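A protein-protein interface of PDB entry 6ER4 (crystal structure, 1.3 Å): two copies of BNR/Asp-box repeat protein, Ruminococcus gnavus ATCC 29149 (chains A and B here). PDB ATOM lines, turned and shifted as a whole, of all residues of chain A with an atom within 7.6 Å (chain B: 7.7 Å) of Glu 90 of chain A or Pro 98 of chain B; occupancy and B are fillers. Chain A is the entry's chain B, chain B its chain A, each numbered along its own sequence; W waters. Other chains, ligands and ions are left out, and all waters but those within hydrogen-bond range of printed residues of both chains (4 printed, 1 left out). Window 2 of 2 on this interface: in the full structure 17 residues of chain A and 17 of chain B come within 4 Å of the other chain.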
ATOM      1  N   ARG A  68     -15.979  28.610 -18.014  1.00  0.00           N
ATOM      2  CA  ARG A  68     -15.769  28.711 -16.580  1.00  0.00           C
ATOM      3  C   ARG A  68     -15.109  30.063 -16.270  1.00  0.00           C
ATOM      4  O   ARG A  68     -13.878  30.217 -16.292  1.00  0.00           O
ATOM      5  CB  ARG A  68     -14.912  27.563 -16.062  1.00  0.00           C
ATOM      6  CG  ARG A  68     -15.483  26.170 -16.394  1.00  0.00           C
ATOM      7  CD  ARG A  68     -14.636  25.104 -15.775  1.00  0.00           C
ATOM      8  NE  ARG A  68     -15.000  23.735 -16.155  1.00  0.00           N
ATOM      9  CZ  ARG A  68     -15.864  22.958 -15.552  1.00  0.00           C
ATOM     10  NH1 ARG A  68     -16.580  23.382 -14.532  1.00  0.00           N
ATOM     11  NH2 ARG A  68     -16.044  21.735 -16.021  1.00  0.00           N
ATOM     12  N   LEU A  84     -21.749  34.889 -14.951  1.00  0.00           N
ATOM     13  CA  LEU A  84     -21.143  34.066 -13.920  1.00  0.00           C
ATOM     14  C   LEU A  84     -21.383  32.631 -14.320  1.00  0.00           C
ATOM     15  O   LEU A  84     -22.523  32.164 -14.349  1.00  0.00           O
ATOM     16  CB  LEU A  84     -21.748  34.415 -12.568  1.00  0.00           C
ATOM     17  CG  LEU A  84     -21.341  33.540 -11.409  1.00  0.00           C
ATOM     18  CD1 LEU A  84     -19.869  33.580 -11.098  1.00  0.00           C
ATOM     19  CD2 LEU A  84     -22.144  33.928 -10.172  1.00  0.00           C
ATOM     20  N   ARG A  85     -20.300  31.944 -14.694  1.00  0.00           N
ATOM     21  CA  ARG A  85     -20.423  30.689 -15.436  1.00  0.00           C
ATOM     22  C   ARG A  85     -19.486  29.599 -14.920  1.00  0.00           C
ATOM     23  O   ARG A  85     -18.303  29.874 -14.601  1.00  0.00           O
ATOM     24  CB  ARG A  85     -20.082  30.916 -16.900  1.00  0.00           C
ATOM     25  CG  ARG A  85     -20.942  31.969 -17.574  1.00  0.00           C
ATOM     26  CD  ARG A  85     -20.758  32.014 -19.076  1.00  0.00           C
ATOM     27  NE  ARG A  85     -21.183  30.746 -19.663  1.00  0.00           N
ATOM     28  CZ  ARG A  85     -21.014  30.405 -20.939  1.00  0.00           C
ATOM     29  NH1 ARG A  85     -20.386  31.234 -21.760  1.00  0.00           N
ATOM     30  NH2 ARG A  85     -21.412  29.225 -21.376  1.00  0.00           N
ATOM     31  N   ASN A  86     -19.977  28.343 -14.863  1.00  0.00           N
ATOM     32  CA  ASN A  86     -19.104  27.205 -14.590  1.00  0.00           C
ATOM     33  C   ASN A  86     -19.467  26.023 -15.444  1.00  0.00           C
ATOM     34  O   ASN A  86     -19.526  24.890 -14.942  1.00  0.00           O
ATOM     35  CB  ASN A  86     -19.087  26.839 -13.106  1.00  0.00           C
ATOM     36  CG  ASN A  86     -17.930  25.932 -12.758  1.00  0.00           C
ATOM     37  OD1 ASN A  86     -16.848  26.080 -13.327  1.00  0.00           O
ATOM     38  ND2 ASN A  86     -18.123  25.025 -11.816  1.00  0.00           N
ATOM     39  N   THR A  87     -19.634  26.293 -16.744  1.00  0.00           N
ATOM     40  CA  THR A  87     -20.352  25.452 -17.720  1.00  0.00           C
ATOM     41  C   THR A  87     -21.858  25.502 -17.457  1.00  0.00           C
ATOM     42  O   THR A  87     -22.300  25.617 -16.291  1.00  0.00           O
ATOM     43  CB  THR A  87     -19.880  23.996 -17.832  1.00  0.00           C
ATOM     44  OG1 THR A  87     -20.387  23.202 -16.759  1.00  0.00           O
ATOM     45  CG2 THR A  87     -18.365  23.864 -17.904  1.00  0.00           C
ATOM     46  N   ASP A  88     -22.631  25.381 -18.526  1.00  0.00           N
ATOM     47  CA  ASP A  88     -24.068  25.588 -18.389  1.00  0.00           C
ATOM     48  C   ASP A  88     -24.771  24.514 -17.543  1.00  0.00           C
ATOM     49  O   ASP A  88     -25.774  24.787 -16.942  1.00  0.00           O
ATOM     50  CB  ASP A  88     -24.720  25.734 -19.759  1.00  0.00           C
ATOM     51  CG  ASP A  88     -24.250  26.958 -20.542  1.00  0.00           C
ATOM     52  OD1 ASP A  88     -23.585  27.823 -19.996  1.00  0.00           O
ATOM     53  OD2 ASP A  88     -24.601  27.011 -21.734  1.00  0.00           O
ATOM     54  N   GLY A  89     -24.194  23.321 -17.506  1.00  0.00           N
ATOM     55  CA  GLY A  89     -24.704  22.244 -16.669  1.00  0.00           C
ATOM     56  C   GLY A  89     -24.602  22.524 -15.179  1.00  0.00           C
ATOM     57  O   GLY A  89     -25.313  21.919 -14.388  1.00  0.00           O
ATOM     58  N   GLU A  90     -23.678  23.402 -14.794  1.00  0.00           N
ATOM     59  CA  GLU A  90     -23.486  23.790 -13.420  1.00  0.00           C
ATOM     60  C   GLU A  90     -24.195  25.093 -13.069  1.00  0.00           C
ATOM     61  O   GLU A  90     -25.047  25.141 -12.193  1.00  0.00           O
ATOM     62  CB  GLU A  90     -21.997  23.890 -13.121  1.00  0.00           C
ATOM     63  CG  GLU A  90     -21.252  22.570 -13.261  1.00  0.00           C
ATOM     64  CD  GLU A  90     -21.653  21.542 -12.230  1.00  0.00           C
ATOM     65  OE1 GLU A  90     -21.664  21.874 -11.036  1.00  0.00           O
ATOM     66  OE2 GLU A  90     -21.976  20.403 -12.619  1.00  0.00           O
ATOM     67  N   PHE A  91     -23.852  26.182 -13.764  1.00  0.00           N
ATOM     68  CA  PHE A  91     -24.589  27.430 -13.633  1.00  0.00           C
ATOM     69  C   PHE A  91     -24.210  28.395 -14.731  1.00  0.00           C
ATOM     70  O   PHE A  91     -23.046  28.445 -15.173  1.00  0.00           O
ATOM     71  CB  PHE A  91     -24.432  28.114 -12.261  1.00  0.00           C
ATOM     72  CG  PHE A  91     -23.032  28.330 -11.761  1.00  0.00           C
ATOM     73  CD1 PHE A  91     -22.338  29.498 -12.048  1.00  0.00           C
ATOM     74  CD2 PHE A  91     -22.422  27.388 -10.918  1.00  0.00           C
ATOM     75  CE1 PHE A  91     -21.078  29.719 -11.524  1.00  0.00           C
ATOM     76  CE2 PHE A  91     -21.142  27.612 -10.409  1.00  0.00           C
ATOM     77  CZ  PHE A  91     -20.480  28.788 -10.705  1.00  0.00           C
ATOM     78  N   LYS A  92     -25.191  29.202 -15.128  1.00  0.00           N
ATOM     79  CA  LYS A  92     -25.000  30.338 -16.024  1.00  0.00           C
ATOM     80  C   LYS A  92     -25.920  31.436 -15.563  1.00  0.00           C
ATOM     81  O   LYS A  92     -27.122  31.431 -15.879  1.00  0.00           O
ATOM     82  CB  LYS A  92     -25.300  29.968 -17.475  1.00  0.00           C
ATOM     83  CG  LYS A  92     -24.937  31.089 -18.434  1.00  0.00           C
ATOM     84  CD  LYS A  92     -25.242  30.830 -19.880  1.00  0.00           C
ATOM     85  CE  LYS A  92     -24.714  31.972 -20.737  1.00  0.00           C
ATOM     86  NZ  LYS A  92     -25.030  31.755 -22.184  1.00  0.00           N
ATOM     87  N   TYR A  93     -25.405  32.324 -14.713  1.00  0.00           N
ATOM     88  CA  TYR A  93     -26.198  33.432 -14.155  1.00  0.00           C
ATOM     89  C   TYR A  93     -25.758  34.720 -14.819  1.00  0.00           C
ATOM     90  O   TYR A  93     -24.562  35.047 -14.829  1.00  0.00           O
ATOM     91  CB  TYR A  93     -25.969  33.555 -12.662  1.00  0.00           C
ATOM     92  CG  TYR A  93     -26.414  32.376 -11.835  1.00  0.00           C
ATOM     93  CD1 TYR A  93     -27.272  31.380 -12.341  1.00  0.00           C
ATOM     94  CD2 TYR A  93     -25.996  32.244 -10.536  1.00  0.00           C
ATOM     95  CE1 TYR A  93     -27.682  30.328 -11.537  1.00  0.00           C
ATOM     96  CE2 TYR A  93     -26.398  31.189  -9.732  1.00  0.00           C
ATOM     97  CZ  TYR A  93     -27.263  30.225 -10.245  1.00  0.00           C
ATOM     98  OH  TYR A  93     -27.677  29.157  -9.476  1.00  0.00           O
ATOM     99  N   GLN A 139     -31.058  34.328  -6.861  1.00  0.00           N
ATOM    100  CA  GLN A 139     -30.997  32.906  -7.276  1.00  0.00           C
ATOM    101  C   GLN A 139     -31.083  32.047  -6.068  1.00  0.00           C
ATOM    102  O   GLN A 139     -30.284  32.230  -5.130  1.00  0.00           O
ATOM    103  CB  GLN A 139     -29.661  32.566  -7.954  1.00  0.00           C
ATOM    104  CG  GLN A 139     -29.520  33.172  -9.295  1.00  0.00           C
ATOM    105  CD  GLN A 139     -30.350  32.611 -10.407  1.00  0.00           C
ATOM    106  OE1 GLN A 139     -30.561  33.349 -11.360  1.00  0.00           O
ATOM    107  NE2 GLN A 139     -30.828  31.328 -10.346  1.00  0.00           N
ATOM    108  N   GLU A 140     -31.940  31.035  -6.102  1.00  0.00           N
ATOM    109  CA  GLU A 140     -32.037  30.134  -4.947  1.00  0.00           C
ATOM    110  C   GLU A 140     -30.729  29.436  -4.682  1.00  0.00           C
ATOM    111  O   GLU A 140     -30.366  29.221  -3.524  1.00  0.00           O
ATOM    112  CB  GLU A 140     -33.172  29.123  -5.142  1.00  0.00           C
ATOM    113  CG  GLU A 140     -33.396  28.229  -3.919  1.00  0.00           C
ATOM    114  CD  GLU A 140     -34.528  27.222  -4.075  1.00  0.00           C
ATOM    115  OE1 GLU A 140     -34.789  26.736  -5.193  1.00  0.00           O
ATOM    116  OE2 GLU A 140     -35.106  26.840  -3.025  1.00  0.00           O
ATOM    117  N   ALA A 141     -30.037  29.059  -5.743  1.00  0.00           N
ATOM    118  CA  ALA A 141     -28.752  28.439  -5.633  1.00  0.00           C
ATOM    119  C   ALA A 141     -27.656  29.506  -5.872  1.00  0.00           C
ATOM    120  O   ALA A 141     -27.112  29.633  -6.962  1.00  0.00           O
ATOM    121  CB  ALA A 141     -28.637  27.279  -6.643  1.00  0.00           C
ATOM    122  N   LYS A 143     -24.305  31.502  -6.243  1.00  0.00           N
ATOM    123  CA  LYS A 143     -22.924  31.156  -6.625  1.00  0.00           C
ATOM    124  C   LYS A 143     -22.086  32.428  -6.702  1.00  0.00           C
ATOM    125  O   LYS A 143     -22.600  33.521  -7.039  1.00  0.00           O
ATOM    126  CB  LYS A 143     -22.897  30.449  -7.971  1.00  0.00           C
ATOM    127  CG  LYS A 143     -23.775  29.198  -8.055  1.00  0.00           C
ATOM    128  CD  LYS A 143     -23.272  28.020  -7.239  1.00  0.00           C
ATOM    129  CE  LYS A 143     -24.262  26.876  -7.330  1.00  0.00           C
ATOM    130  NZ  LYS A 143     -23.809  25.769  -6.466  1.00  0.00           N
ATOM    131  N   ASP A 147     -17.092  29.346  -6.589  1.00  0.00           N
ATOM    132  CA  ASP A 147     -17.770  28.180  -7.125  1.00  0.00           C
ATOM    133  C   ASP A 147     -17.354  27.827  -8.543  1.00  0.00           C
ATOM    134  O   ASP A 147     -17.722  26.764  -9.048  1.00  0.00           O
ATOM    135  CB  ASP A 147     -19.272  28.382  -7.084  1.00  0.00           C
ATOM    136  CG  ASP A 147     -19.776  28.588  -5.699  1.00  0.00           C
ATOM    137  OD1 ASP A 147     -19.650  27.639  -4.898  1.00  0.00           O
ATOM    138  OD2 ASP A 147     -20.286  29.669  -5.399  1.00  0.00           O
ATOM    139  N   THR A 149     -14.831  26.404 -11.251  1.00  0.00           N
ATOM    140  CA  THR A 149     -13.808  25.362 -11.153  1.00  0.00           C
ATOM    141  C   THR A 149     -12.519  25.798 -11.853  1.00  0.00           C
ATOM    142  O   THR A 149     -12.528  26.135 -13.052  1.00  0.00           O
ATOM    143  CB  THR A 149     -14.320  24.061 -11.770  1.00  0.00           C
ATOM    144  OG1 THR A 149     -15.531  23.683 -11.099  1.00  0.00           O
ATOM    145  CG2 THR A 149     -13.295  22.962 -11.644  1.00  0.00           C
ATOM    146  N   THR B  75     -33.998  22.181 -19.677  1.00  0.00           N
ATOM    147  CA  THR B  75     -32.801  21.633 -20.281  1.00  0.00           C
ATOM    148  C   THR B  75     -32.608  20.184 -19.932  1.00  0.00           C
ATOM    149  O   THR B  75     -33.170  19.679 -18.968  1.00  0.00           O
ATOM    150  CB  THR B  75     -31.537  22.396 -19.864  1.00  0.00           C
ATOM    151  OG1 THR B  75     -31.121  21.989 -18.552  1.00  0.00           O
ATOM    152  CG2 THR B  75     -31.768  23.909 -19.962  1.00  0.00           C
ATOM    153  N   ALA B  77     -30.033  19.032 -18.564  1.00  0.00           N
ATOM    154  CA  ALA B  77     -29.275  18.947 -17.320  1.00  0.00           C
ATOM    155  C   ALA B  77     -30.168  19.245 -16.111  1.00  0.00           C
ATOM    156  O   ALA B  77     -29.649  19.442 -15.025  1.00  0.00           O
ATOM    157  CB  ALA B  77     -28.123  19.932 -17.374  1.00  0.00           C
ATOM    158  N   GLY B  78     -31.495  19.293 -16.303  1.00  0.00           N
ATOM    159  CA  GLY B  78     -32.417  19.573 -15.217  1.00  0.00           C
ATOM    160  C   GLY B  78     -32.605  21.063 -14.914  1.00  0.00           C
ATOM    161  O   GLY B  78     -33.069  21.420 -13.839  1.00  0.00           O
ATOM    162  N   GLY B  79     -32.255  21.914 -15.853  1.00  0.00           N
ATOM    163  CA  GLY B  79     -32.400  23.333 -15.697  1.00  0.00           C
ATOM    164  C   GLY B  79     -33.759  23.814 -16.176  1.00  0.00           C
ATOM    165  O   GLY B  79     -34.440  23.178 -16.974  1.00  0.00           O
ATOM    166  N   VAL B  80     -34.138  24.977 -15.671  1.00  0.00           N
ATOM    167  CA  VAL B  80     -35.334  25.719 -16.112  1.00  0.00           C
ATOM    168  C   VAL B  80     -34.877  27.131 -16.400  1.00  0.00           C
ATOM    169  O   VAL B  80     -34.097  27.696 -15.638  1.00  0.00           O
ATOM    170  CB  VAL B  80     -36.439  25.710 -15.035  1.00  0.00           C
ATOM    171  CG1 VAL B  80     -37.706  26.430 -15.511  1.00  0.00           C
ATOM    172  CG2 VAL B  80     -36.799  24.325 -14.582  1.00  0.00           C
ATOM    173  N   GLY B  81     -35.403  27.701 -17.484  1.00  0.00           N
ATOM    174  CA  GLY B  81     -35.090  29.078 -17.797  1.00  0.00           C
ATOM    175  C   GLY B  81     -36.129  29.778 -18.615  1.00  0.00           C
ATOM    176  O   GLY B  81     -37.115  29.196 -19.024  1.00  0.00           O
ATOM    177  N   ASP B  96     -31.803  31.326 -15.934  1.00  0.00           N
ATOM    178  CA  ASP B  96     -31.368  29.948 -16.101  1.00  0.00           C
ATOM    179  C   ASP B  96     -31.015  29.409 -14.731  1.00  0.00           C
ATOM    180  O   ASP B  96     -30.122  29.957 -14.063  1.00  0.00           O
ATOM    181  CB  ASP B  96     -30.185  29.864 -17.059  1.00  0.00           C
ATOM    182  CG  ASP B  96     -30.055  28.542 -17.630  1.00  0.00           C
ATOM    183  OD1 ASP B  96     -29.449  27.719 -16.932  1.00  0.00           O
ATOM    184  OD2 ASP B  96     -30.624  28.284 -18.720  1.00  0.00           O
ATOM    185  N   CYS B  97     -31.753  28.391 -14.289  1.00  0.00           N
ATOM    186  CA  CYS B  97     -31.649  27.868 -12.916  1.00  0.00           C
ATOM    187  C   CYS B  97     -31.281  26.425 -12.979  1.00  0.00           C
ATOM    188  O   CYS B  97     -32.016  25.623 -13.601  1.00  0.00           O
ATOM    189  CB  CYS B  97     -32.972  27.989 -12.178  1.00  0.00           C
ATOM    190  SG  CYS B  97     -33.531  29.682 -12.074  1.00  0.00           S
ATOM    191  N   PRO B  98     -30.208  26.018 -12.291  1.00  0.00           N
ATOM    192  CA  PRO B  98     -29.780  24.615 -12.370  1.00  0.00           C
ATOM    193  C   PRO B  98     -30.527  23.721 -11.411  1.00  0.00           C
ATOM    194  O   PRO B  98     -31.017  24.161 -10.372  1.00  0.00           O
ATOM    195  CB  PRO B  98     -28.315  24.688 -11.924  1.00  0.00           C
ATOM    196  CG  PRO B  98     -28.271  25.806 -10.961  1.00  0.00           C
ATOM    197  CD  PRO B  98     -29.230  26.825 -11.532  1.00  0.00           C
ATOM    198  N   ALA B  99     -30.558  22.440 -11.773  1.00  0.00           N
ATOM    199  CA  ALA B  99     -30.988  21.391 -10.842  1.00  0.00           C
ATOM    200  C   ALA B  99     -32.366  21.649 -10.236  1.00  0.00           C
ATOM    201  O   ALA B  99     -32.597  21.461  -9.044  1.00  0.00           O
ATOM    202  CB  ALA B  99     -29.921  21.191  -9.763  1.00  0.00           C
ATOM    203  N   ALA B 100     -33.281  22.101 -11.090  1.00  0.00           N
ATOM    204  CA  ALA B 100     -34.613  22.476 -10.677  1.00  0.00           C
ATOM    205  C   ALA B 100     -35.719  21.500 -11.093  1.00  0.00           C
ATOM    206  O   ALA B 100     -36.792  21.471 -10.480  1.00  0.00           O
ATOM    207  CB  ALA B 100     -34.918  23.885 -11.185  1.00  0.00           C
ATOM    208  N   VAL B 101     -35.467  20.718 -12.143  1.00  0.00           N
ATOM    209  CA  VAL B 101     -36.416  19.722 -12.687  1.00  0.00           C
ATOM    210  C   VAL B 101     -35.615  18.448 -12.956  1.00  0.00           C
ATOM    211  O   VAL B 101     -34.375  18.452 -12.965  1.00  0.00           O
ATOM    212  CB  VAL B 101     -37.137  20.209 -13.959  1.00  0.00           C
ATOM    213  CG1 VAL B 101     -38.103  21.344 -13.606  1.00  0.00           C
ATOM    214  CG2 VAL B 101     -36.167  20.589 -15.059  1.00  0.00           C
ATOM    215  N   ILE B 134     -37.426  29.730  -7.607  1.00  0.00           N
ATOM    216  CA  ILE B 134     -36.052  29.430  -7.921  1.00  0.00           C
ATOM    217  C   ILE B 134     -35.235  30.634  -8.395  1.00  0.00           C
ATOM    218  O   ILE B 134     -34.002  30.618  -8.310  1.00  0.00           O
ATOM    219  CB  ILE B 134     -35.935  28.234  -8.911  1.00  0.00           C
ATOM    220  CG1 ILE B 134     -36.617  28.476 -10.247  1.00  0.00           C
ATOM    221  CG2 ILE B 134     -36.454  26.948  -8.261  1.00  0.00           C
ATOM    222  CD1 ILE B 134     -36.473  27.323 -11.253  1.00  0.00           C
HETATM  223  O   HOH W   1     -30.275  32.719 -13.859  1.00  0.00           O
HETATM  224  O   HOH W   2     -27.305  26.667 -17.792  1.00  0.00           O
HETATM  225  O   HOH W   3     -28.676  21.765 -13.912  1.00  0.00           O
HETATM  226  O   HOH W   4     -27.809  28.347 -14.420  1.00  0.00           O
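NE2 of Gln 139 of chain A lies within hydrogen-bond range of SG of Cys 97 of chain B, at 3.6 Å.
The backbone carbonyl oxygen (O) of Ile 134 of chain B lies within hydrogen-bond range of the backbone NH (N) of Glu 140 of chain A, 3.0 Å away.
N of Cys 97 of chain B sits at hydrogen-bond distance from O of Val 80 of chain B, at 2.8 Å.
The backbone carbonyl oxygen of Tyr 93 of chain A lies within hydrogen-bond range of the backbone NH of Leu 84 of chain A (2.8 Å).
The side-chain hydroxyl (OH) of Tyr 93 of chain A sits at hydrogen-bond distance from the backbone carbonyl oxygen (O) of Ala 141 of chain A, at 2.6 Å.
Pro 98 of chain B touches Glu 90 of chain A (CB to O, 3.3 Å).
Asp 96 of chain B touches Lys 92 of chain A (CB to O, 3.6 Å).
Tyr 93 of chain A touches Asp 96 of chain B (CE1 to O, 3.5 Å).
Pro 98 of chain B touches Tyr 93 of chain A.
O of Ile 134 of chain B touches NE2 of Gln 139 of chain A, 3.8 Å away.
Arg 85 of chain A touches none of the printed residues of chain B.
Gly 89 of chain A touches none of the printed residues of chain B.
Of the printed residues of chain B, Glu 90 of chain A touches Pro 98 (3.3 Å).
Printed residues of chain B within 4 Å of Lys 92 of chain A: Asp 96.
Printed residues of chain B within 4 Å of Tyr 93 of chain A: Asp 96 (3.5 Å) and Pro 98 (3.5 Å).
Printed residues of chain B within 4 Å of Gln 139 of chain A: Cys 97 and Ile 134.
Of the printed residues of chain B, Glu 140 of chain A touches Ile 134.
Of the printed residues of chain A, Asp 96 of chain B touches Lys 92 and Tyr 93.
Of chain A, only Glu 90 and Tyr 93 come within 4 Å of Pro 98 of chain B.
No residue of chain A comes within 4 Å of Ala 99 of chain B.
Of the 13 printed residues of chain B, 4 touch a printed residue of chain A.
Among the printed residues, no Asp or Glu carboxylate lies within 4 Å of a Lys or Arg side-chain nitrogen of the other chain.
No position is printed for both chains.
Water W2 lies within hydrogen-bond range of the side-chain carboxylate of Asp 96 of chain B (2.5 Å) and the backbone carbonyl oxygen of Asp 88 of chain A (2.6 Å).
Water W1 lies within hydrogen-bond range of OE1 of Gln 139 of chain A (2.6 Å) and O of Asp 96 of chain B (2.8 Å).
Water W3 lies within hydrogen-bond range of O of Ala 77 of chain B (2.8 Å), N of Ala 99 of chain B (2.9 Å) and O of Gly 89 of chain A (3.4 Å).
Water W4 lies within hydrogen-bond range of the backbone carbonyl oxygen of Asp 96 of chain B (2.8 Å) and the backbone NH of Lys 92 of chain A (2.8 Å).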
